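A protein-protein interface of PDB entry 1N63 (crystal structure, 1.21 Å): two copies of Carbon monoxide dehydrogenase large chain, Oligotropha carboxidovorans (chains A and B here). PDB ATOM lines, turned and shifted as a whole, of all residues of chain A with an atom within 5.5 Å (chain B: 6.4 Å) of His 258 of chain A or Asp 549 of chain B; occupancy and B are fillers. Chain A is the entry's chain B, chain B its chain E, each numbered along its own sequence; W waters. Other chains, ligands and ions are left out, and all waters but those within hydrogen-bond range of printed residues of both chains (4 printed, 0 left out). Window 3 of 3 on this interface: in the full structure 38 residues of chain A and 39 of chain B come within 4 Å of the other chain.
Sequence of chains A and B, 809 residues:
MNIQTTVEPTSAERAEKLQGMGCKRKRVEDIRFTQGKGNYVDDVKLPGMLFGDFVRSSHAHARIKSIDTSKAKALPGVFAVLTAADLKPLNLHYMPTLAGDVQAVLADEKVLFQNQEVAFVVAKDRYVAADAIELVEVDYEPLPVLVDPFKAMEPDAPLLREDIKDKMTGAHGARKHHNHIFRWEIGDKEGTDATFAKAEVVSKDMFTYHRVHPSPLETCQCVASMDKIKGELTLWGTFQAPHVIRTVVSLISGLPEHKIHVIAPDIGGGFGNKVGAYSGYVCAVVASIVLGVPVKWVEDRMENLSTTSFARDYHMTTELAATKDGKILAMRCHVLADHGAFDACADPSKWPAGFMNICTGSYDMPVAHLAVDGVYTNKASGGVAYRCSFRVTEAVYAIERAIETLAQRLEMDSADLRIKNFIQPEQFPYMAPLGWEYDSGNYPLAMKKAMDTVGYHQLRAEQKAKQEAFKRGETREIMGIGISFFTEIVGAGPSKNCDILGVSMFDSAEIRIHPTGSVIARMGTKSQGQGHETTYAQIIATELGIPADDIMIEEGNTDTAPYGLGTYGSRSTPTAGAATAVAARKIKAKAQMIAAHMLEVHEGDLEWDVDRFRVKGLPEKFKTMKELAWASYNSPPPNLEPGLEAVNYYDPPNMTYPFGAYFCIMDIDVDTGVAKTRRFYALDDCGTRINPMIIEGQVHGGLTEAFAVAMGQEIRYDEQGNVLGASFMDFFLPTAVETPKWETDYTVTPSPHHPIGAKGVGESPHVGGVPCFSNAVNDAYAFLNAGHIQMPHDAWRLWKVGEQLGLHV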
ATOM      1  N   GLU A 232     -13.751  17.259 -39.401  1.00  0.00           N
ATOM      2  CA  GLU A 232     -15.178  16.877 -39.408  1.00  0.00           C
ATOM      3  C   GLU A 232     -15.732  16.927 -40.820  1.00  0.00           C
ATOM      4  O   GLU A 232     -15.523  17.888 -41.574  1.00  0.00           O
ATOM      5  CB  GLU A 232     -16.034  17.832 -38.565  1.00  0.00           C
ATOM      6  CG  GLU A 232     -15.649  17.805 -37.097  1.00  0.00           C
ATOM      7  CD  GLU A 232     -16.342  18.839 -36.250  1.00  0.00           C
ATOM      8  OE1 GLU A 232     -17.506  19.144 -36.604  1.00  0.00           O
ATOM      9  OE2 GLU A 232     -15.772  19.216 -35.202  1.00  0.00           O
ATOM     10  N   PRO A 256     -14.789   9.063 -36.886  1.00  0.00           N
ATOM     11  CA  PRO A 256     -15.745   8.630 -35.859  1.00  0.00           C
ATOM     12  C   PRO A 256     -17.077   9.326 -36.117  1.00  0.00           C
ATOM     13  O   PRO A 256     -17.150  10.395 -36.751  1.00  0.00           O
ATOM     14  CB  PRO A 256     -15.086   9.086 -34.553  1.00  0.00           C
ATOM     15  CG  PRO A 256     -14.275  10.319 -34.975  1.00  0.00           C
ATOM     16  CD  PRO A 256     -13.788  10.006 -36.350  1.00  0.00           C
ATOM     17  N   GLU A 257     -18.158   8.697 -35.665  1.00  0.00           N
ATOM     18  CA  GLU A 257     -19.486   9.131 -35.981  1.00  0.00           C
ATOM     19  C   GLU A 257     -19.828  10.530 -35.487  1.00  0.00           C
ATOM     20  O   GLU A 257     -20.663  11.233 -36.118  1.00  0.00           O
ATOM     21  CB  GLU A 257     -20.516   8.101 -35.537  1.00  0.00           C
ATOM     22  CG  GLU A 257     -20.606   6.859 -36.374  1.00  0.00           C
ATOM     23  CD  GLU A 257     -21.719   5.942 -35.947  1.00  0.00           C
ATOM     24  OE1 GLU A 257     -22.858   6.242 -36.379  1.00  0.00           O
ATOM     25  OE2 GLU A 257     -21.515   5.079 -35.056  1.00  0.00           O
ATOM     26  N   HIS A 258     -19.240  10.963 -34.373  1.00  0.00           N
ATOM     27  CA  HIS A 258     -19.553  12.293 -33.839  1.00  0.00           C
ATOM     28  C   HIS A 258     -18.851  13.380 -34.679  1.00  0.00           C
ATOM     29  O   HIS A 258     -19.180  14.539 -34.479  1.00  0.00           O
ATOM     30  CB  HIS A 258     -19.152  12.414 -32.357  1.00  0.00           C
ATOM     31  CG  HIS A 258     -17.691  12.292 -32.149  1.00  0.00           C
ATOM     32  ND1 HIS A 258     -16.922  13.106 -31.337  1.00  0.00           N
ATOM     33  CD2 HIS A 258     -16.874  11.325 -32.590  1.00  0.00           C
ATOM     34  CE1 HIS A 258     -15.661  12.664 -31.356  1.00  0.00           C
ATOM     35  NE2 HIS A 258     -15.622  11.574 -32.096  1.00  0.00           N
ATOM     36  N   LYS A 259     -18.013  12.980 -35.625  1.00  0.00           N
ATOM     37  CA  LYS A 259     -17.367  13.897 -36.531  1.00  0.00           C
ATOM     38  C   LYS A 259     -17.837  13.774 -37.962  1.00  0.00           C
ATOM     39  O   LYS A 259     -17.221  14.290 -38.868  1.00  0.00           O
ATOM     40  CB  LYS A 259     -15.840  13.837 -36.386  1.00  0.00           C
ATOM     41  CG  LYS A 259     -15.432  14.309 -34.988  1.00  0.00           C
ATOM     42  CD  LYS A 259     -13.977  14.425 -34.724  1.00  0.00           C
ATOM     43  CE  LYS A 259     -13.716  14.927 -33.287  1.00  0.00           C
ATOM     44  NZ  LYS A 259     -12.292  15.022 -33.059  1.00  0.00           N
ATOM     45  N   ILE A 260     -18.921  13.048 -38.134  1.00  0.00           N
ATOM     46  CA  ILE A 260     -19.563  12.933 -39.461  1.00  0.00           C
ATOM     47  C   ILE A 260     -21.004  13.412 -39.341  1.00  0.00           C
ATOM     48  O   ILE A 260     -21.788  12.857 -38.579  1.00  0.00           O
ATOM     49  CB  ILE A 260     -19.595  11.479 -39.974  1.00  0.00           C
ATOM     50  CG1 ILE A 260     -18.182  10.873 -40.033  1.00  0.00           C
ATOM     51  CG2 ILE A 260     -20.308  11.430 -41.322  1.00  0.00           C
ATOM     52  CD1 ILE A 260     -18.209   9.407 -40.257  1.00  0.00           C
ATOM     53  N   HIS A 261     -21.299  14.529 -39.981  1.00  0.00           N
ATOM     54  CA  HIS A 261     -22.604  15.201 -39.891  1.00  0.00           C
ATOM     55  C   HIS A 261     -23.313  14.955 -41.192  1.00  0.00           C
ATOM     56  O   HIS A 261     -23.082  15.642 -42.186  1.00  0.00           O
ATOM     57  CB  HIS A 261     -22.358  16.696 -39.674  1.00  0.00           C
ATOM     58  CG  HIS A 261     -21.320  16.985 -38.605  1.00  0.00           C
ATOM     59  ND1 HIS A 261     -21.453  16.533 -37.302  1.00  0.00           N
ATOM     60  CD2 HIS A 261     -20.118  17.605 -38.651  1.00  0.00           C
ATOM     61  CE1 HIS A 261     -20.382  16.878 -36.606  1.00  0.00           C
ATOM     62  NE2 HIS A 261     -19.569  17.551 -37.403  1.00  0.00           N
ATOM     63  N   ASP A 559     -26.938  14.571 -36.561  1.00  0.00           N
ATOM     64  CA  ASP A 559     -26.448  15.143 -35.317  1.00  0.00           C
ATOM     65  C   ASP A 559     -27.631  15.349 -34.337  1.00  0.00           C
ATOM     66  O   ASP A 559     -27.419  15.385 -33.116  1.00  0.00           O
ATOM     67  CB  ASP A 559     -25.891  16.571 -35.553  1.00  0.00           C
ATOM     68  CG  ASP A 559     -24.504  16.634 -36.125  1.00  0.00           C
ATOM     69  OD1 ASP A 559     -23.859  15.611 -36.382  1.00  0.00           O
ATOM     70  OD2 ASP A 559     -24.020  17.756 -36.387  1.00  0.00           O
ATOM     71  N   LYS B  17      -5.507   8.014 -23.682  1.00  0.00           N
ATOM     72  CA  LYS B  17      -6.563   8.599 -24.497  1.00  0.00           C
ATOM     73  C   LYS B  17      -7.715   9.165 -23.648  1.00  0.00           C
ATOM     74  O   LYS B  17      -8.531   9.939 -24.150  1.00  0.00           O
ATOM     75  N   LEU B  18      -7.816   8.801 -22.367  1.00  0.00           N
ATOM     76  CA  LEU B  18      -9.085   9.074 -21.645  1.00  0.00           C
ATOM     77  C   LEU B  18      -9.354  10.598 -21.440  1.00  0.00           C
ATOM     78  O   LEU B  18     -10.437  11.117 -21.786  1.00  0.00           O
ATOM     79  CB  LEU B  18      -9.225   8.326 -20.303  1.00  0.00           C
ATOM     80  CG  LEU B  18     -10.631   8.369 -19.712  1.00  0.00           C
ATOM     81  CD1 LEU B  18     -11.634   7.512 -20.564  1.00  0.00           C
ATOM     82  CD2 LEU B  18     -10.616   7.954 -18.241  1.00  0.00           C
ATOM     83  N   GLN B  19      -8.381  11.306 -20.868  1.00  0.00           N
ATOM     84  CA  GLN B  19      -8.472  12.758 -20.625  1.00  0.00           C
ATOM     85  C   GLN B  19      -9.716  13.188 -19.878  1.00  0.00           C
ATOM     86  O   GLN B  19     -10.415  14.162 -20.247  1.00  0.00           O
ATOM     87  CB  GLN B  19      -8.367  13.532 -21.950  1.00  0.00           C
ATOM     88  CG  GLN B  19      -7.220  13.075 -22.834  1.00  0.00           C
ATOM     89  CD  GLN B  19      -5.971  13.913 -22.652  1.00  0.00           C
ATOM     90  OE1 GLN B  19      -4.917  13.378 -22.324  1.00  0.00           O
ATOM     91  NE2 GLN B  19      -6.108  15.227 -22.763  1.00  0.00           N
ATOM     92  N   ARG B  25      -6.596  18.772 -19.739  1.00  0.00           N
ATOM     93  CA  ARG B  25      -6.885  18.529 -21.137  1.00  0.00           C
ATOM     94  C   ARG B  25      -6.815  19.816 -21.926  1.00  0.00           C
ATOM     95  O   ARG B  25      -7.407  20.852 -21.526  1.00  0.00           O
ATOM     96  CB  ARG B  25      -8.299  17.926 -21.215  1.00  0.00           C
ATOM     97  CG  ARG B  25      -8.690  17.549 -22.627  1.00  0.00           C
ATOM     98  CD  ARG B  25     -10.119  17.053 -22.808  1.00  0.00           C
ATOM     99  NE  ARG B  25     -10.339  16.727 -24.212  1.00  0.00           N
ATOM    100  CZ  ARG B  25     -11.500  16.764 -24.841  1.00  0.00           C
ATOM    101  NH1 ARG B  25     -12.581  17.265 -24.282  1.00  0.00           N
ATOM    102  NH2 ARG B  25     -11.541  16.357 -26.088  1.00  0.00           N
ATOM    103  N   LYS B  26      -6.071  19.779 -23.029  1.00  0.00           N
ATOM    104  CA  LYS B  26      -5.965  20.919 -23.902  1.00  0.00           C
ATOM    105  C   LYS B  26      -7.285  21.144 -24.632  1.00  0.00           C
ATOM    106  O   LYS B  26      -8.049  20.220 -24.848  1.00  0.00           O
ATOM    107  CB  LYS B  26      -4.814  20.741 -24.882  1.00  0.00           C
ATOM    108  CG  LYS B  26      -3.459  20.542 -24.191  1.00  0.00           C
ATOM    109  CD  LYS B  26      -3.107  21.749 -23.337  1.00  0.00           C
ATOM    110  CE  LYS B  26      -2.091  21.430 -22.220  1.00  0.00           C
ATOM    111  NZ  LYS B  26      -0.671  21.366 -22.656  1.00  0.00           N
ATOM    112  N   VAL B  28     -10.358  21.914 -26.979  1.00  0.00           N
ATOM    113  CA  VAL B  28     -10.772  21.625 -28.341  1.00  0.00           C
ATOM    114  C   VAL B  28     -11.138  22.887 -29.121  1.00  0.00           C
ATOM    115  O   VAL B  28     -10.934  22.947 -30.342  1.00  0.00           O
ATOM    116  CB  VAL B  28     -11.951  20.605 -28.423  1.00  0.00           C
ATOM    117  CG1 VAL B  28     -11.523  19.258 -27.844  1.00  0.00           C
ATOM    118  CG2 VAL B  28     -13.171  21.104 -27.700  1.00  0.00           C
ATOM    119  N   HIS B 514     -23.381   6.734 -29.872  1.00  0.00           N
ATOM    120  CA  HIS B 514     -23.565   6.195 -31.211  1.00  0.00           C
ATOM    121  C   HIS B 514     -23.167   4.713 -31.234  1.00  0.00           C
ATOM    122  O   HIS B 514     -22.535   4.224 -30.285  1.00  0.00           O
ATOM    123  CB  HIS B 514     -22.675   6.948 -32.190  1.00  0.00           C
ATOM    124  CG  HIS B 514     -23.071   8.384 -32.325  1.00  0.00           C
ATOM    125  ND1 HIS B 514     -24.381   8.821 -32.267  1.00  0.00           N
ATOM    126  CD2 HIS B 514     -22.296   9.479 -32.514  1.00  0.00           C
ATOM    127  CE1 HIS B 514     -24.379  10.133 -32.416  1.00  0.00           C
ATOM    128  NE2 HIS B 514     -23.143  10.558 -32.556  1.00  0.00           N
ATOM    129  N   SER B 518     -18.762   6.615 -30.074  1.00  0.00           N
ATOM    130  CA  SER B 518     -18.586   8.039 -29.905  1.00  0.00           C
ATOM    131  C   SER B 518     -19.899   8.627 -29.420  1.00  0.00           C
ATOM    132  O   SER B 518     -20.927   7.946 -29.326  1.00  0.00           O
ATOM    133  CB  SER B 518     -18.083   8.639 -31.188  1.00  0.00           C
ATOM    134  OG  SER B 518     -18.981   8.382 -32.282  1.00  0.00           O
ATOM    135  N   VAL B 519     -19.870   9.911 -29.099  1.00  0.00           N
ATOM    136  CA  VAL B 519     -20.910  10.556 -28.307  1.00  0.00           C
ATOM    137  C   VAL B 519     -21.198  11.987 -28.788  1.00  0.00           C
ATOM    138  O   VAL B 519     -20.232  12.703 -29.083  1.00  0.00           O
ATOM    139  CB  VAL B 519     -20.425  10.617 -26.848  1.00  0.00           C
ATOM    140  CG1 VAL B 519     -21.520  11.249 -25.966  1.00  0.00           C
ATOM    141  CG2 VAL B 519     -20.109   9.263 -26.289  1.00  0.00           C
ATOM    142  N   ILE B 520     -22.484  12.343 -28.820  1.00  0.00           N
ATOM    143  CA  ILE B 520     -22.891  13.751 -28.928  1.00  0.00           C
ATOM    144  C   ILE B 520     -23.596  14.089 -27.614  1.00  0.00           C
ATOM    145  O   ILE B 520     -24.507  13.370 -27.203  1.00  0.00           O
ATOM    146  CB  ILE B 520     -23.749  14.000 -30.191  1.00  0.00           C
ATOM    147  CG1 ILE B 520     -24.258  15.427 -30.217  1.00  0.00           C
ATOM    148  CG2 ILE B 520     -24.961  13.093 -30.314  1.00  0.00           C
ATOM    149  CD1 ILE B 520     -23.197  16.442 -30.369  1.00  0.00           C
ATOM    150  N   ALA B 537     -16.943  17.208 -21.549  1.00  0.00           N
ATOM    151  CA  ALA B 537     -16.528  15.905 -22.037  1.00  0.00           C
ATOM    152  C   ALA B 537     -15.648  15.149 -21.043  1.00  0.00           C
ATOM    153  O   ALA B 537     -15.707  13.927 -21.014  1.00  0.00           O
ATOM    154  CB  ALA B 537     -15.769  16.053 -23.355  1.00  0.00           C
ATOM    155  N   ILE B 546     -15.146   6.521 -21.708  1.00  0.00           N
ATOM    156  CA  ILE B 546     -15.049   6.818 -23.151  1.00  0.00           C
ATOM    157  C   ILE B 546     -14.058   7.984 -23.241  1.00  0.00           C
ATOM    158  O   ILE B 546     -14.257   9.020 -22.648  1.00  0.00           O
ATOM    159  CB  ILE B 546     -16.438   7.238 -23.674  1.00  0.00           C
ATOM    160  CG1 ILE B 546     -17.408   6.034 -23.631  1.00  0.00           C
ATOM    161  CG2 ILE B 546     -16.305   7.818 -25.100  1.00  0.00           C
ATOM    162  CD1 ILE B 546     -18.823   6.405 -23.992  1.00  0.00           C
ATOM    163  N   PRO B 547     -13.091   7.910 -24.150  1.00  0.00           N
ATOM    164  CA  PRO B 547     -12.116   8.988 -24.236  1.00  0.00           C
ATOM    165  C   PRO B 547     -12.839  10.309 -24.508  1.00  0.00           C
ATOM    166  O   PRO B 547     -13.695  10.388 -25.413  1.00  0.00           O
ATOM    167  CB  PRO B 547     -11.281   8.588 -25.453  1.00  0.00           C
ATOM    168  CG  PRO B 547     -11.361   7.143 -25.532  1.00  0.00           C
ATOM    169  CD  PRO B 547     -12.725   6.748 -24.964  1.00  0.00           C
ATOM    170  N   ALA B 548     -12.259  11.390 -23.995  1.00  0.00           N
ATOM    171  CA  ALA B 548     -12.901  12.690 -24.174  1.00  0.00           C
ATOM    172  C   ALA B 548     -12.943  13.081 -25.629  1.00  0.00           C
ATOM    173  O   ALA B 548     -13.868  13.753 -26.049  1.00  0.00           O
ATOM    174  CB  ALA B 548     -12.166  13.718 -23.336  1.00  0.00           C
ATOM    175  N   ASP B 549     -11.938  12.742 -26.429  1.00  0.00           N
ATOM    176  CA  ASP B 549     -11.936  13.123 -27.853  1.00  0.00           C
ATOM    177  C   ASP B 549     -12.993  12.389 -28.647  1.00  0.00           C
ATOM    178  O   ASP B 549     -13.253  12.764 -29.777  1.00  0.00           O
ATOM    179  CB  ASP B 549     -10.576  12.942 -28.491  1.00  0.00           C
ATOM    180  CG  ASP B 549      -9.617  13.983 -28.038  1.00  0.00           C
ATOM    181  OD1 ASP B 549      -9.995  15.206 -28.193  1.00  0.00           O
ATOM    182  OD2 ASP B 549      -8.436  13.609 -27.908  1.00  0.00           O
ATOM    183  N   ASP B 550     -13.587  11.331 -28.098  1.00  0.00           N
ATOM    184  CA  ASP B 550     -14.690  10.643 -28.732  1.00  0.00           C
ATOM    185  C   ASP B 550     -16.071  11.236 -28.404  1.00  0.00           C
ATOM    186  O   ASP B 550     -17.104  10.671 -28.761  1.00  0.00           O
ATOM    187  CB  ASP B 550     -14.698   9.157 -28.330  1.00  0.00           C
ATOM    188  CG  ASP B 550     -13.505   8.386 -28.758  1.00  0.00           C
ATOM    189  OD1 ASP B 550     -12.648   8.915 -29.519  1.00  0.00           O
ATOM    190  OD2 ASP B 550     -13.379   7.187 -28.377  1.00  0.00           O
ATOM    191  N   ILE B 551     -16.059  12.397 -27.782  1.00  0.00           N
ATOM    192  CA  ILE B 551     -17.261  13.060 -27.300  1.00  0.00           C
ATOM    193  C   ILE B 551     -17.302  14.455 -27.902  1.00  0.00           C
ATOM    194  O   ILE B 551     -16.357  15.216 -27.757  1.00  0.00           O
ATOM    195  CB  ILE B 551     -17.235  13.146 -25.751  1.00  0.00           C
ATOM    196  CG1 ILE B 551     -17.046  11.732 -25.163  1.00  0.00           C
ATOM    197  CG2 ILE B 551     -18.496  13.871 -25.205  1.00  0.00           C
ATOM    198  CD1 ILE B 551     -16.829  11.652 -23.631  1.00  0.00           C
ATOM    199  N   MET B 552     -18.421  14.794 -28.512  1.00  0.00           N
ATOM    200  CA  MET B 552     -18.674  16.150 -29.027  1.00  0.00           C
ATOM    201  C   MET B 552     -19.594  16.871 -28.068  1.00  0.00           C
ATOM    202  O   MET B 552     -20.672  16.348 -27.831  1.00  0.00           O
ATOM    203  CB  MET B 552     -19.337  16.079 -30.412  1.00  0.00           C
ATOM    204  CG  MET B 552     -20.002  17.343 -30.874  1.00  0.00           C
ATOM    205  SD  MET B 552     -19.514  17.676 -32.576  1.00  0.00           S
ATOM    206  CE  MET B 552     -17.853  18.186 -32.218  1.00  0.00           C
HETATM  207  O   HOH W   1     -12.153  15.955 -30.371  1.00  0.00           O
HETATM  208  O   HOH W   2     -21.549  15.285 -33.329  1.00  0.00           O
HETATM  209  O   HOH W   3     -17.567   6.557 -33.717  1.00  0.00           O
HETATM  210  O   HOH W   4     -22.077  17.885 -34.014  1.00  0.00           O
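No position is printed for both chains.
Of the 10 pairs that touch across the chains among the printed residues, none has its exchanged pair printed and touching as well.
Printed residues of chain B that touch a printed residue of chain A: His 514, Ser 518, Val 519, Asp 549, Asp 550, Ile 551 and Met 552.
Hydrophobic or aromatic side chains of chain B that line the printed part of chain A: His 514 and Met 552.
Along chain B the printed residues that touch a printed residue of chain A span positions 514 to 552.
Among the printed residues, merely in contact across the chains: His 258 of chain A with Asp 549 of chain B (2.9 Å), His 258 of chain A with Asp 550 of chain B (3.3 Å), His 258 of chain A with Val 519 of chain B (3.5 Å), His 258 of chain A with Ile 551 of chain B (3.6 Å), Glu 257 of chain A with His 514 of chain B (3.6 Å), Glu 232 of chain A with Met 552 of chain B (3.8 Å) and His 258 of chain A with His 514 of chain B (3.9 Å).
Of the printed residues of chain B, His 258 of chain A touches His 514, Ser 518, Val 519, Asp 549, Asp 550, Ile 551 and Met 552.
Val 28 of chain B touches none of the printed residues of chain A.
Of the printed residues of chain A, Val 519 of chain B touches His 258 (3.5 Å).
Of the printed residues of chain A, Asp 549 of chain B touches His 258 (2.9 Å).
Printed residues of chain A within 4 Å of Asp 550 of chain B: His 258.
The nearest printed residue of chain B that does not touch His 258 of chain A is Ile 520 of chain B (4.9 Å).
The nearest residue of chain A that does not touch Asp 549 of chain B is Lys 259 of chain A (4.1 Å).
The nearest printed residue of chain B that does not touch Glu 257 of chain A is Val 519 of chain B (6.4 Å).
The backbone NH (N) of Val 519 of chain B sits at hydrogen-bond distance from the backbone carbonyl oxygen (O) of Asp 550 of chain B, at 2.9 Å.
A ring nitrogen (NE2) of His 261 of chain A lies within hydrogen-bond range of the side-chain carboxylate (OE1) of Glu 232 of chain A, at 2.7 Å.
The backbone NH (N) of Met 552 of chain B sits at hydrogen-bond distance from the backbone carbonyl oxygen (O) of Val 519 of chain B, 2.8 Å away.
NH2 of Arg 25 of chain B lies within salt-bridge range of OD1 of Asp 549 of chain B, 2.9 Å away.
N of Glu 257 of chain A lies within hydrogen-bond range of OG of Ser 518 of chain B, 3.5 Å away.
The backbone NH of His 258 of chain A lies within hydrogen-bond range of the side-chain hydroxyl of Ser 518 of chain B (3.3 Å).
SD of Met 552 of chain B lies close to O of His 258 of chain A.
Water W3 lies within hydrogen-bond range of OG of Ser 518 of chain B (2.7 Å) and N of Glu 257 of chain A (3.0 Å).
Water W2 lies within hydrogen-bond range of the backbone carbonyl oxygen of His 258 of chain A (2.7 Å) and the side-chain sulfur of Met 552 of chain B (3.2 Å).
Water W1 bridges NZ of Lys 259 of chain A (2.8 Å) and OD1 of Asp 549 of chain B (3.2 Å).
Water W4 lies within hydrogen-bond range of SD of Met 552 of chain B (2.9 Å) and OD2 of Asp 559 of chain A (3.1 Å).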
